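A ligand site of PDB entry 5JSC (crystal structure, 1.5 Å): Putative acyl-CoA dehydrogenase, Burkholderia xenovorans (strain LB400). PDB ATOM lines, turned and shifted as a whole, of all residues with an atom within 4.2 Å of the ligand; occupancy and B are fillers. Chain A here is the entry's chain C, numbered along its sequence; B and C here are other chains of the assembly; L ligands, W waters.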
ATOM      1  N   MET A 111      33.677  17.359  -7.306  1.00  0.00           N
ATOM      2  CA  MET A 111      34.612  16.959  -6.260  1.00  0.00           C
ATOM      3  C   MET A 111      35.988  17.580  -6.433  1.00  0.00           C
ATOM      4  O   MET A 111      36.701  17.721  -5.439  1.00  0.00           O
ATOM      5  CB  MET A 111      34.733  15.437  -6.206  1.00  0.00           C
ATOM      6  CG  MET A 111      33.472  14.773  -5.681  1.00  0.00           C
ATOM      7  SD  MET A 111      32.866  15.502  -4.142  1.00  0.00           S
ATOM      8  CE  MET A 111      34.354  15.456  -3.119  1.00  0.00           C
ATOM      9  N   PHE A 144      36.974  15.260   0.108  1.00  0.00           N
ATOM     10  CA  PHE A 144      36.593  16.093   1.250  1.00  0.00           C
ATOM     11  C   PHE A 144      36.042  15.141   2.310  1.00  0.00           C
ATOM     12  O   PHE A 144      34.952  14.589   2.137  1.00  0.00           O
ATOM     13  CB  PHE A 144      35.532  17.098   0.795  1.00  0.00           C
ATOM     14  CG  PHE A 144      35.051  18.070   1.856  1.00  0.00           C
ATOM     15  CD1 PHE A 144      35.770  19.217   2.148  1.00  0.00           C
ATOM     16  CD2 PHE A 144      33.822  17.877   2.485  1.00  0.00           C
ATOM     17  CE1 PHE A 144      35.316  20.132   3.075  1.00  0.00           C
ATOM     18  CE2 PHE A 144      33.351  18.793   3.412  1.00  0.00           C
ATOM     19  CZ  PHE A 144      34.097  19.919   3.714  1.00  0.00           C
ATOM     20  N   ALA A 145      36.796  14.924   3.374  1.00  0.00           N
ATOM     21  CA  ALA A 145      36.471  13.861   4.344  1.00  0.00           C
ATOM     22  C   ALA A 145      36.035  14.484   5.682  1.00  0.00           C
ATOM     23  O   ALA A 145      36.867  14.743   6.566  1.00  0.00           O
ATOM     24  CB  ALA A 145      37.648  12.891   4.532  1.00  0.00           C
ATOM     25  N   LEU A 146      34.731  14.672   5.836  1.00  0.00           N
ATOM     26  CA  LEU A 146      34.125  15.318   6.992  1.00  0.00           C
ATOM     27  C   LEU A 146      33.220  14.372   7.757  1.00  0.00           C
ATOM     28  O   LEU A 146      33.380  14.227   8.985  1.00  0.00           O
ATOM     29  CB  LEU A 146      33.332  16.550   6.521  1.00  0.00           C
ATOM     30  CG  LEU A 146      32.681  17.404   7.616  1.00  0.00           C
ATOM     31  CD1 LEU A 146      33.761  17.945   8.550  1.00  0.00           C
ATOM     32  CD2 LEU A 146      31.856  18.542   7.001  1.00  0.00           C
ATOM     33  N   SER A 147      32.297  13.708   7.072  1.00  0.00           N
ATOM     34  CA  SER A 147      31.290  12.865   7.702  1.00  0.00           C
ATOM     35  C   SER A 147      31.888  11.587   8.286  1.00  0.00           C
ATOM     36  O   SER A 147      32.873  11.039   7.786  1.00  0.00           O
ATOM     37  CB  SER A 147      30.222  12.490   6.675  1.00  0.00           C
ATOM     38  OG  SER A 147      29.616  13.651   6.146  1.00  0.00           O
ATOM     39  N   ALA A 151      28.322  10.484  12.838  1.00  0.00           N
ATOM     40  CA  ALA A 151      28.097  11.928  12.826  1.00  0.00           C
ATOM     41  C   ALA A 151      28.298  12.474  11.427  1.00  0.00           C
ATOM     42  O   ALA A 151      29.437  12.557  10.948  1.00  0.00           O
ATOM     43  CB  ALA A 151      29.029  12.626  13.821  1.00  0.00           C
ATOM     44  N   GLY A 152      27.208  12.876  10.781  1.00  0.00           N
ATOM     45  CA  GLY A 152      27.243  13.564   9.498  1.00  0.00           C
ATOM     46  C   GLY A 152      26.684  14.962   9.625  1.00  0.00           C
ATOM     47  O   GLY A 152      27.394  15.945   9.357  1.00  0.00           O
ATOM     48  N   SER A 153      25.425  15.084  10.048  1.00  0.00           N
ATOM     49  CA  SER A 153      24.865  16.408  10.316  1.00  0.00           C
ATOM     50  C   SER A 153      25.568  17.093  11.492  1.00  0.00           C
ATOM     51  O   SER A 153      25.838  18.293  11.448  1.00  0.00           O
ATOM     52  CB  SER A 153      23.368  16.300  10.608  1.00  0.00           C
ATOM     53  OG  SER A 153      22.697  15.686   9.519  1.00  0.00           O
ATOM     54  N   TRP A 177      31.014   7.755   3.743  1.00  0.00           N
ATOM     55  CA  TRP A 177      30.314   8.390   2.615  1.00  0.00           C
ATOM     56  C   TRP A 177      31.253   9.311   1.844  1.00  0.00           C
ATOM     57  O   TRP A 177      30.819  10.339   1.319  1.00  0.00           O
ATOM     58  CB  TRP A 177      29.073   9.192   3.046  1.00  0.00           C
ATOM     59  CG  TRP A 177      28.211   8.541   4.094  1.00  0.00           C
ATOM     60  CD1 TRP A 177      27.990   8.990   5.375  1.00  0.00           C
ATOM     61  CD2 TRP A 177      27.468   7.326   3.958  1.00  0.00           C
ATOM     62  NE1 TRP A 177      27.154   8.115   6.037  1.00  0.00           N
ATOM     63  CE2 TRP A 177      26.820   7.095   5.189  1.00  0.00           C
ATOM     64  CE3 TRP A 177      27.282   6.416   2.918  1.00  0.00           C
ATOM     65  CZ2 TRP A 177      26.015   5.976   5.417  1.00  0.00           C
ATOM     66  CZ3 TRP A 177      26.478   5.314   3.128  1.00  0.00           C
ATOM     67  CH2 TRP A 177      25.859   5.099   4.372  1.00  0.00           C
ATOM     68  N   ILE A 178      32.535   8.968   1.763  1.00  0.00           N
ATOM     69  CA  ILE A 178      33.512   9.902   1.224  1.00  0.00           C
ATOM     70  C   ILE A 178      33.541   9.770  -0.296  1.00  0.00           C
ATOM     71  O   ILE A 178      33.943   8.744  -0.837  1.00  0.00           O
ATOM     72  CB  ILE A 178      34.913   9.665   1.824  1.00  0.00           C
ATOM     73  CG1 ILE A 178      34.859   9.842   3.342  1.00  0.00           C
ATOM     74  CG2 ILE A 178      35.917  10.640   1.195  1.00  0.00           C
ATOM     75  CD1 ILE A 178      34.131  11.107   3.794  1.00  0.00           C
ATOM     76  N   SER A 179      33.093  10.830  -0.981  1.00  0.00           N
ATOM     77  CA  SER A 179      33.120  10.876  -2.437  1.00  0.00           C
ATOM     78  C   SER A 179      34.555  10.770  -2.954  1.00  0.00           C
ATOM     79  O   SER A 179      35.471  11.405  -2.410  1.00  0.00           O
ATOM     80  CB  SER A 179      32.481  12.165  -2.931  1.00  0.00           C
ATOM     81  OG  SER A 179      31.096  12.180  -2.645  1.00  0.00           O
ATOM     82  N   LEU A 228      32.647   5.936  -3.760  1.00  0.00           N
ATOM     83  CA  LEU A 228      32.402   6.277  -2.364  1.00  0.00           C
ATOM     84  C   LEU A 228      33.104   5.257  -1.483  1.00  0.00           C
ATOM     85  O   LEU A 228      33.158   4.073  -1.815  1.00  0.00           O
ATOM     86  CB  LEU A 228      30.900   6.289  -2.030  1.00  0.00           C
ATOM     87  CG  LEU A 228      30.010   7.476  -2.384  1.00  0.00           C
ATOM     88  CD1 LEU A 228      28.554   7.074  -2.172  1.00  0.00           C
ATOM     89  CD2 LEU A 228      30.371   8.654  -1.512  1.00  0.00           C
ATOM     90  N   ALA A 377      20.088  11.624  -3.473  1.00  0.00           N
ATOM     91  CA  ALA A 377      21.172  11.941  -2.558  1.00  0.00           C
ATOM     92  C   ALA A 377      21.428  13.441  -2.430  1.00  0.00           C
ATOM     93  O   ALA A 377      21.996  13.861  -1.413  1.00  0.00           O
ATOM     94  CB  ALA A 377      22.472  11.265  -2.996  1.00  0.00           C
ATOM     95  N   ILE A 380      20.506  15.196   0.653  1.00  0.00           N
ATOM     96  CA  ILE A 380      21.170  14.658   1.836  1.00  0.00           C
ATOM     97  C   ILE A 380      22.600  15.175   1.958  1.00  0.00           C
ATOM     98  O   ILE A 380      22.999  15.682   3.016  1.00  0.00           O
ATOM     99  CB  ILE A 380      21.129  13.114   1.849  1.00  0.00           C
ATOM    100  CG1 ILE A 380      19.681  12.629   1.934  1.00  0.00           C
ATOM    101  CG2 ILE A 380      21.959  12.554   3.017  1.00  0.00           C
ATOM    102  CD1 ILE A 380      19.472  11.185   1.522  1.00  0.00           C
ATOM    103  N   TYR A 381      23.372  15.093   0.878  1.00  0.00           N
ATOM    104  CA  TYR A 381      24.770  15.477   1.012  1.00  0.00           C
ATOM    105  C   TYR A 381      24.933  16.999   0.916  1.00  0.00           C
ATOM    106  O   TYR A 381      24.027  17.727   0.506  1.00  0.00           O
ATOM    107  CB  TYR A 381      25.651  14.723   0.018  1.00  0.00           C
ATOM    108  CG  TYR A 381      25.563  14.965  -1.496  1.00  0.00           C
ATOM    109  CD1 TYR A 381      25.682  16.245  -2.036  1.00  0.00           C
ATOM    110  CD2 TYR A 381      25.487  13.890  -2.382  1.00  0.00           C
ATOM    111  CE1 TYR A 381      25.671  16.443  -3.422  1.00  0.00           C
ATOM    112  CE2 TYR A 381      25.493  14.086  -3.767  1.00  0.00           C
ATOM    113  CZ  TYR A 381      25.582  15.363  -4.272  1.00  0.00           C
ATOM    114  OH  TYR A 381      25.601  15.586  -5.634  1.00  0.00           O
ATOM    115  N   GLU A 382      26.124  17.464   1.347  1.00  0.00           N
ATOM    116  CA  GLU A 382      26.443  18.874   1.599  1.00  0.00           C
ATOM    117  C   GLU A 382      25.412  19.522   2.537  1.00  0.00           C
ATOM    118  O   GLU A 382      25.150  20.726   2.463  1.00  0.00           O
ATOM    119  CB  GLU A 382      26.618  19.672   0.293  1.00  0.00           C
ATOM    120  CG  GLU A 382      27.876  19.265  -0.534  1.00  0.00           C
ATOM    121  CD  GLU A 382      28.504  20.399  -1.350  1.00  0.00           C
ATOM    122  OE1 GLU A 382      28.460  21.573  -0.911  1.00  0.00           O
ATOM    123  OE2 GLU A 382      29.063  20.122  -2.448  1.00  0.00           O
ATOM    124  N   ALA A 384      21.784  18.074   4.851  1.00  0.00           N
ATOM    125  CA  ALA A 384      20.448  17.621   4.486  1.00  0.00           C
ATOM    126  C   ALA A 384      19.473  18.801   4.458  1.00  0.00           C
ATOM    127  O   ALA A 384      19.690  19.843   5.073  1.00  0.00           O
ATOM    128  CB  ALA A 384      19.966  16.559   5.481  1.00  0.00           C
ATOM    129  N   GLU A 386      16.818  19.418   5.964  1.00  0.00           N
ATOM    130  CA  GLU A 386      16.386  19.908   7.264  1.00  0.00           C
ATOM    131  C   GLU A 386      17.454  20.772   7.914  1.00  0.00           C
ATOM    132  O   GLU A 386      17.128  21.745   8.612  1.00  0.00           O
ATOM    133  CB  GLU A 386      16.013  18.711   8.159  1.00  0.00           C
ATOM    134  CG  GLU A 386      14.768  17.915   7.648  1.00  0.00           C
ATOM    135  CD  GLU A 386      14.984  17.183   6.317  1.00  0.00           C
ATOM    136  OE1 GLU A 386      16.103  16.692   6.072  1.00  0.00           O
ATOM    137  OE2 GLU A 386      14.011  17.089   5.527  1.00  0.00           O
ATOM    138  N   VAL A 387      18.733  20.452   7.693  1.00  0.00           N
ATOM    139  CA  VAL A 387      19.815  21.313   8.158  1.00  0.00           C
ATOM    140  C   VAL A 387      19.738  22.673   7.480  1.00  0.00           C
ATOM    141  O   VAL A 387      19.879  23.716   8.138  1.00  0.00           O
ATOM    142  CB  VAL A 387      21.182  20.629   7.911  1.00  0.00           C
ATOM    143  CG1 VAL A 387      22.323  21.580   8.227  1.00  0.00           C
ATOM    144  CG2 VAL A 387      21.298  19.358   8.718  1.00  0.00           C
ATOM    145  N   LEU A 390      16.893  24.838   8.990  1.00  0.00           N
ATOM    146  CA  LEU A 390      17.207  25.410  10.284  1.00  0.00           C
ATOM    147  C   LEU A 390      18.230  26.530  10.174  1.00  0.00           C
ATOM    148  O   LEU A 390      18.152  27.502  10.930  1.00  0.00           O
ATOM    149  CB  LEU A 390      17.684  24.312  11.231  1.00  0.00           C
ATOM    150  CG  LEU A 390      16.654  23.230  11.551  1.00  0.00           C
ATOM    151  CD1 LEU A 390      17.327  22.066  12.257  1.00  0.00           C
ATOM    152  CD2 LEU A 390      15.522  23.815  12.387  1.00  0.00           C
ATOM    153  N   ARG B 287      19.262   6.947  16.615  1.00  0.00           N
ATOM    154  CA  ARG B 287      20.331   7.765  16.047  1.00  0.00           C
ATOM    155  C   ARG B 287      20.683   8.905  16.995  1.00  0.00           C
ATOM    156  O   ARG B 287      19.905   9.849  17.149  1.00  0.00           O
ATOM    157  CB  ARG B 287      19.906   8.300  14.678  1.00  0.00           C
ATOM    158  CG  ARG B 287      21.000   9.116  13.992  1.00  0.00           C
ATOM    159  CD  ARG B 287      22.207   8.259  13.684  1.00  0.00           C
ATOM    160  NE  ARG B 287      23.116   8.932  12.761  1.00  0.00           N
ATOM    161  CZ  ARG B 287      24.275   8.415  12.342  1.00  0.00           C
ATOM    162  NH1 ARG B 287      24.679   7.234  12.771  1.00  0.00           N
ATOM    163  NH2 ARG B 287      25.028   9.106  11.478  1.00  0.00           N
ATOM    164  N   MET B 289      22.481  12.278  18.122  1.00  0.00           N
ATOM    165  CA  MET B 289      22.938  13.492  17.463  1.00  0.00           C
ATOM    166  C   MET B 289      22.629  14.681  18.354  1.00  0.00           C
ATOM    167  O   MET B 289      21.609  14.704  19.050  1.00  0.00           O
ATOM    168  CB  MET B 289      22.290  13.679  16.078  1.00  0.00           C
ATOM    169  CG  MET B 289      20.773  13.665  16.103  1.00  0.00           C
ATOM    170  SD  MET B 289      20.029  14.342  14.610  1.00  0.00           S
ATOM    171  CE  MET B 289      20.643  13.219  13.335  1.00  0.00           C
ATOM    172  N   PHE B 290      23.533  15.664  18.334  1.00  0.00           N
ATOM    173  CA  PHE B 290      23.324  16.948  19.020  1.00  0.00           C
ATOM    174  C   PHE B 290      22.980  16.729  20.491  1.00  0.00           C
ATOM    175  O   PHE B 290      22.147  17.427  21.074  1.00  0.00           O
ATOM    176  CB  PHE B 290      22.256  17.784  18.305  1.00  0.00           C
ATOM    177  CG  PHE B 290      22.593  18.086  16.871  1.00  0.00           C
ATOM    178  CD1 PHE B 290      23.529  19.057  16.555  1.00  0.00           C
ATOM    179  CD2 PHE B 290      21.990  17.380  15.839  1.00  0.00           C
ATOM    180  CE1 PHE B 290      23.852  19.340  15.248  1.00  0.00           C
ATOM    181  CE2 PHE B 290      22.296  17.658  14.508  1.00  0.00           C
ATOM    182  CZ  PHE B 290      23.232  18.635  14.215  1.00  0.00           C
ATOM    183  N   LEU B 294      17.755  11.718  17.266  1.00  0.00           N
ATOM    184  CA  LEU B 294      17.011  12.285  16.147  1.00  0.00           C
ATOM    185  C   LEU B 294      15.531  12.467  16.492  1.00  0.00           C
ATOM    186  O   LEU B 294      14.926  13.494  16.153  1.00  0.00           O
ATOM    187  CB  LEU B 294      17.197  11.385  14.922  1.00  0.00           C
ATOM    188  CG  LEU B 294      16.481  11.704  13.609  1.00  0.00           C
ATOM    189  CD1 LEU B 294      16.787  13.127  13.129  1.00  0.00           C
ATOM    190  CD2 LEU B 294      16.896  10.686  12.556  1.00  0.00           C
ATOM    191  N   PHE B 297      13.918  15.732  18.296  1.00  0.00           N
ATOM    192  CA  PHE B 297      13.695  16.974  17.573  1.00  0.00           C
ATOM    193  C   PHE B 297      12.257  17.095  17.087  1.00  0.00           C
ATOM    194  O   PHE B 297      11.690  16.130  16.571  1.00  0.00           O
ATOM    195  CB  PHE B 297      14.635  17.051  16.388  1.00  0.00           C
ATOM    196  CG  PHE B 297      16.040  17.415  16.760  1.00  0.00           C
ATOM    197  CD1 PHE B 297      16.324  18.674  17.269  1.00  0.00           C
ATOM    198  CD2 PHE B 297      17.076  16.520  16.546  1.00  0.00           C
ATOM    199  CE1 PHE B 297      17.614  19.028  17.576  1.00  0.00           C
ATOM    200  CE2 PHE B 297      18.390  16.878  16.848  1.00  0.00           C
ATOM    201  CZ  PHE B 297      18.656  18.134  17.371  1.00  0.00           C
ATOM    202  N   THR B 300      11.517  15.894  13.553  1.00  0.00           N
ATOM    203  CA  THR B 300      11.420  14.449  13.423  1.00  0.00           C
ATOM    204  C   THR B 300      10.071  13.958  13.913  1.00  0.00           C
ATOM    205  O   THR B 300       9.438  13.114  13.282  1.00  0.00           O
ATOM    206  CB  THR B 300      12.543  13.765  14.204  1.00  0.00           C
ATOM    207  OG1 THR B 300      13.811  14.255  13.748  1.00  0.00           O
ATOM    208  CG2 THR B 300      12.477  12.255  14.027  1.00  0.00           C
ATOM    209  N   GLN B 355      14.968   9.960   4.174  1.00  0.00           N
ATOM    210  CA  GLN B 355      15.574  11.193   4.693  1.00  0.00           C
ATOM    211  C   GLN B 355      16.043  11.024   6.129  1.00  0.00           C
ATOM    212  O   GLN B 355      17.131  11.487   6.498  1.00  0.00           O
ATOM    213  CB  GLN B 355      14.575  12.345   4.576  1.00  0.00           C
ATOM    214  CG  GLN B 355      15.205  13.711   4.700  1.00  0.00           C
ATOM    215  CD  GLN B 355      16.060  14.104   3.499  1.00  0.00           C
ATOM    216  OE1 GLN B 355      16.095  13.418   2.476  1.00  0.00           O
ATOM    217  NE2 GLN B 355      16.757  15.232   3.623  1.00  0.00           N
ATOM    218  N   LEU B 356      15.244  10.326   6.953  1.00  0.00           N
ATOM    219  CA  LEU B 356      15.636  10.106   8.343  1.00  0.00           C
ATOM    220  C   LEU B 356      16.935   9.321   8.454  1.00  0.00           C
ATOM    221  O   LEU B 356      17.685   9.505   9.425  1.00  0.00           O
ATOM    222  CB  LEU B 356      14.517   9.357   9.084  1.00  0.00           C
ATOM    223  CG  LEU B 356      13.242  10.158   9.389  1.00  0.00           C
ATOM    224  CD1 LEU B 356      12.127   9.209   9.831  1.00  0.00           C
ATOM    225  CD2 LEU B 356      13.518  11.207  10.449  1.00  0.00           C
ATOM    226  N   GLY B 358      19.520   9.570   6.455  1.00  0.00           N
ATOM    227  CA  GLY B 358      20.703  10.279   5.977  1.00  0.00           C
ATOM    228  C   GLY B 358      21.337   9.529   4.822  1.00  0.00           C
ATOM    229  O   GLY B 358      20.642   8.947   3.969  1.00  0.00           O
ATOM    230  N   GLY B 359      22.674   9.528   4.781  1.00  0.00           N
ATOM    231  CA  GLY B 359      23.372   8.891   3.682  1.00  0.00           C
ATOM    232  C   GLY B 359      23.014   7.418   3.521  1.00  0.00           C
ATOM    233  O   GLY B 359      22.916   6.901   2.410  1.00  0.00           O
ATOM    234  N   VAL B 362      20.198   6.140   1.006  1.00  0.00           N
ATOM    235  CA  VAL B 362      20.406   5.854  -0.413  1.00  0.00           C
ATOM    236  C   VAL B 362      21.435   4.743  -0.614  1.00  0.00           C
ATOM    237  O   VAL B 362      21.832   4.467  -1.745  1.00  0.00           O
ATOM    238  CB  VAL B 362      20.776   7.120  -1.207  1.00  0.00           C
ATOM    239  CG1 VAL B 362      19.634   8.132  -1.191  1.00  0.00           C
ATOM    240  CG2 VAL B 362      22.069   7.748  -0.683  1.00  0.00           C
ATOM    241  N   GLN C 298      11.688  24.206  16.910  1.00  0.00           N
ATOM    242  CA  GLN C 298      12.059  23.841  15.540  1.00  0.00           C
ATOM    243  C   GLN C 298      10.928  24.060  14.561  1.00  0.00           C
ATOM    244  O   GLN C 298      11.159  24.495  13.426  1.00  0.00           O
ATOM    245  CB  GLN C 298      12.487  22.383  15.458  1.00  0.00           C
ATOM    246  CG  GLN C 298      13.929  22.167  15.661  1.00  0.00           C
ATOM    247  CD  GLN C 298      14.410  20.821  15.142  1.00  0.00           C
ATOM    248  OE1 GLN C 298      13.621  19.879  14.920  1.00  0.00           O
ATOM    249  NE2 GLN C 298      15.707  20.712  14.951  1.00  0.00           N
HETATM  250  P1  LIG L   1      22.292  12.089  10.134  1.00  0.00           P
HETATM  251  O1  LIG L   1      23.246  13.128  10.580  1.00  0.00           O
HETATM  252  O2  LIG L   1      22.081  10.881  11.052  1.00  0.00           O
HETATM  253  O3  LIG L   1      20.905  12.804   9.839  1.00  0.00           O
HETATM  254  C1  LIG L   1      19.750  11.999   9.490  1.00  0.00           C
HETATM  255  C2  LIG L   1      18.669  12.982   9.117  1.00  0.00           C
HETATM  256  O4  LIG L   1      18.313  13.753  10.279  1.00  0.00           O
HETATM  257  C3  LIG L   1      19.070  14.045   8.105  1.00  0.00           C
HETATM  258  O5  LIG L   1      19.081  13.563   6.757  1.00  0.00           O
HETATM  259  C4  LIG L   1      18.027  15.133   8.358  1.00  0.00           C
HETATM  260  O6  LIG L   1      16.820  14.826   7.656  1.00  0.00           O
HETATM  261  C5  LIG L   1      17.792  14.998   9.871  1.00  0.00           C
HETATM  262  N1  LIG L   1      18.399  16.031  10.694  1.00  0.00           N
HETATM  263  C6  LIG L   1      19.736  16.350  10.787  1.00  0.00           C
HETATM  264  N2  LIG L   1      20.011  17.260  11.675  1.00  0.00           N
HETATM  265  C7  LIG L   1      18.775  17.585  12.215  1.00  0.00           C
HETATM  266  C8  LIG L   1      18.382  18.481  13.227  1.00  0.00           C
HETATM  267  N3  LIG L   1      19.231  19.274  13.887  1.00  0.00           N
HETATM  268  N4  LIG L   1      17.069  18.548  13.538  1.00  0.00           N
HETATM  269  C9  LIG L   1      16.204  17.774  12.861  1.00  0.00           C
HETATM  270  N5  LIG L   1      16.458  16.888  11.884  1.00  0.00           N
HETATM  271  C10 LIG L   1      17.777  16.838  11.616  1.00  0.00           C
HETATM  272  N6  LIG L   1      30.325  13.414   3.404  1.00  0.00           N
HETATM  273  C11 LIG L   1      31.618  13.842   3.342  1.00  0.00           C
HETATM  274  O7  LIG L   1      32.251  14.193   4.363  1.00  0.00           O
HETATM  275  N7  LIG L   1      32.272  13.888   2.133  1.00  0.00           N
HETATM  276  C12 LIG L   1      31.734  13.527   0.920  1.00  0.00           C
HETATM  277  O8  LIG L   1      32.423  13.519  -0.091  1.00  0.00           O
HETATM  278  C13 LIG L   1      30.360  13.109   0.975  1.00  0.00           C
HETATM  279  N8  LIG L   1      29.799  12.691  -0.122  1.00  0.00           N
HETATM  280  C14 LIG L   1      28.553  12.091  -0.034  1.00  0.00           C
HETATM  281  C15 LIG L   1      28.011  11.500  -1.171  1.00  0.00           C
HETATM  282  C16 LIG L   1      26.805  10.801  -1.117  1.00  0.00           C
HETATM  283  C17 LIG L   1      26.278  10.138  -2.363  1.00  0.00           C
HETATM  284  C18 LIG L   1      26.119  10.708   0.100  1.00  0.00           C
HETATM  285  C19 LIG L   1      24.817   9.956   0.210  1.00  0.00           C
HETATM  286  C20 LIG L   1      26.650  11.315   1.242  1.00  0.00           C
HETATM  287  C21 LIG L   1      27.867  11.998   1.184  1.00  0.00           C
HETATM  288  N9  LIG L   1      28.474  12.529   2.336  1.00  0.00           N
HETATM  289  C22 LIG L   1      29.734  13.070   2.275  1.00  0.00           C
HETATM  290  C23 LIG L   1      27.806  12.377   3.640  1.00  0.00           C
HETATM  291  C24 LIG L   1      26.678  13.368   3.863  1.00  0.00           C
HETATM  292  O9  LIG L   1      27.183  14.684   4.050  1.00  0.00           O
HETATM  293  C25 LIG L   1      25.879  12.952   5.104  1.00  0.00           C
HETATM  294  O10 LIG L   1      25.220  11.740   4.744  1.00  0.00           O
HETATM  295  C26 LIG L   1      24.854  13.987   5.556  1.00  0.00           C
HETATM  296  O11 LIG L   1      25.544  15.100   6.139  1.00  0.00           O
HETATM  297  C27 LIG L   1      23.869  13.404   6.553  1.00  0.00           C
HETATM  298  O12 LIG L   1      24.626  12.861   7.658  1.00  0.00           O
HETATM  299  P2  LIG L   1      24.212  11.366   8.143  1.00  0.00           P
HETATM  300  O13 LIG L   1      24.158  10.426   6.988  1.00  0.00           O
HETATM  301  O14 LIG L   1      25.115  10.951   9.266  1.00  0.00           O
HETATM  302  O15 LIG L   1      22.728  11.538   8.706  1.00  0.00           O
HETATM  303  O   HOH W   1      28.883  16.248   1.968  1.00  0.00           O
HETATM  304  O   HOH W   2      28.281  17.797   4.811  1.00  0.00           O
HETATM  305  O   HOH W   3      14.390  14.043   8.539  1.00  0.00           O
HETATM  306  O   HOH W   4      20.189   8.833  10.457  1.00  0.00           O
HETATM  307  O   HOH W   5      24.917  13.562  12.735  1.00  0.00           O
HETATM  308  O   HOH W   6      14.246  15.257  11.096  1.00  0.00           O
HETATM  309  O   HOH W   7      35.047  13.541  -0.756  1.00  0.00           O
HETATM  310  O   HOH W   8      19.529  21.454  15.898  1.00  0.00           O
HETATM  311  O   HOH W   9      23.576   7.776   7.460  1.00  0.00           O
HETATM  312  O   HOH W  10      23.492  16.928   6.982  1.00  0.00           O
HETATM  313  O   HOH W  11      26.880   8.951   8.829  1.00  0.00           O
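Water W11 lies within hydrogen-bond range of an oxygen (O14) of the ligand (2.7 Å), the indole nitrogen (NE1) of Trp 177 (2.9 Å) and the guanidinium group (NH2) of Arg 287 of chain B (3.2 Å). Water W9 lies within hydrogen-bond range of O13 of the ligand (2.8 Å) and N of Gly 359 of chain B (3.3 Å). Water W4 lies within hydrogen-bond range of O of Leu 356 of chain B (2.8 Å) and O2 of the ligand (2.9 Å). Water W6 bridges a nitrogen (N5) of the ligand (2.9 Å) and the side-chain hydroxyl of Thr 300 of chain B (2.9 Å). Water W10 lies within hydrogen-bond range of an oxygen (O11) of the ligand, the side-chain hydroxyl (OG) of Ser 153 and the backbone NH (N) of Ala 384. Water W1 lies within hydrogen-bond range of the backbone NH of Glu 382 (3.1 Å) and an oxygen (O9) of the ligand (3.1 Å).
The backbone carbonyl oxygen of Leu 294 of chain B lies within hydrogen-bond range of the side-chain hydroxyl of Thr 300 of chain B (2.8 Å). The backbone NH (N) of Leu 294 of chain B lies within hydrogen-bond range of the backbone carbonyl oxygen (O) of Arg 287 of chain B, at 2.9 Å. The side-chain carboxylate (OE1) of Glu 386 lies within hydrogen-bond range of the side-chain amide nitrogen (NE2) of Gln 355 of chain B.
O of Trp 177 lies close to N8 of the ligand. Merely in contact with the ligand: Leu 356 of chain B, Leu 294 of chain B, Ala 384, Phe 290 of chain B, Met 289 of chain B, Phe 297 of chain B, Ile 380, Tyr 381, Gly 358 of chain B, Val 362 of chain B, Ile 178, Leu 228, Leu 390 and Val 387. Hydrophobic or aromatic side chains that line the ligand: Leu 146, Trp 177, Ile 178, Leu 228, Ile 380, Tyr 381, Ala 384, Val 387, Leu 390, Met 289 of chain B, Phe 290 of chain B, Leu 294 of chain B, Phe 297 of chain B and Val 362 of chain B. 26 residues have an atom within 4 Å of the ligand: Phe 144, Leu 146, Ser 147, Gly 152, Ser 153, Trp 177, Ile 178, Ser 179, Leu 228, Ile 380, Tyr 381, Ala 384, Glu 386, Val 387, Leu 390, Arg 287 of chain B, Met 289 of chain B, Phe 290 of chain B, Leu 294 of chain B, Phe 297 of chain B, Gln 355 of chain B, Leu 356 of chain B, Gly 358 of chain B, Gly 359 of chain B, Val 362 of chain B and Gln 298 of chain C. The nearest printed residue that does not touch the ligand is Ala 145 (4.02 Å).
N of Leu 146 is in hydrogen-bond range of O7 of the ligand, 2.9 Å away. O6 of the ligand is in hydrogen-bond range of OE1 of Glu 386 (2.6 Å). O1 of the ligand is in hydrogen-bond range of OG of Ser 153 (2.8 Å). N of Ser 153 is in hydrogen-bond range of O1 of the ligand (3.0 Å). O of Phe 144 sits at hydrogen-bond distance from N7 of the ligand. An oxygen (O5) of the ligand lies within hydrogen-bond range of the backbone carbonyl oxygen (O) of Gln 355 of chain B (2.9 Å). A nitrogen (N8) of the ligand is in hydrogen-bond range of the side-chain hydroxyl (OG) of Ser 179 (2.9 Å). A nitrogen (N4) of the ligand sits at hydrogen-bond distance from the side-chain amide nitrogen (NE2) of Gln 298 of chain C (2.9 Å). A nitrogen (N6) of the ligand is in hydrogen-bond range of the side-chain hydroxyl (OG) of Ser 147 (2.8 Å). The backbone NH (N) of Gly 152 sits at hydrogen-bond distance from an oxygen (O14) of the ligand, at 3.2 Å. The backbone NH of Gly 359 of chain B is in hydrogen-bond range of an oxygen (O13) of the ligand (2.8 Å). O2 of the ligand is in salt-bridge range of NE of Arg 287 of chain B, at 2.8 Å. The backbone NH (N) of Ser 179 sits at hydrogen-bond distance from an oxygen (O8) of the ligand (2.9 Å). The backbone NH (N) of Ser 147 lies within hydrogen-bond range of an oxygen (O7) of the ligand, at 2.8 Å.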
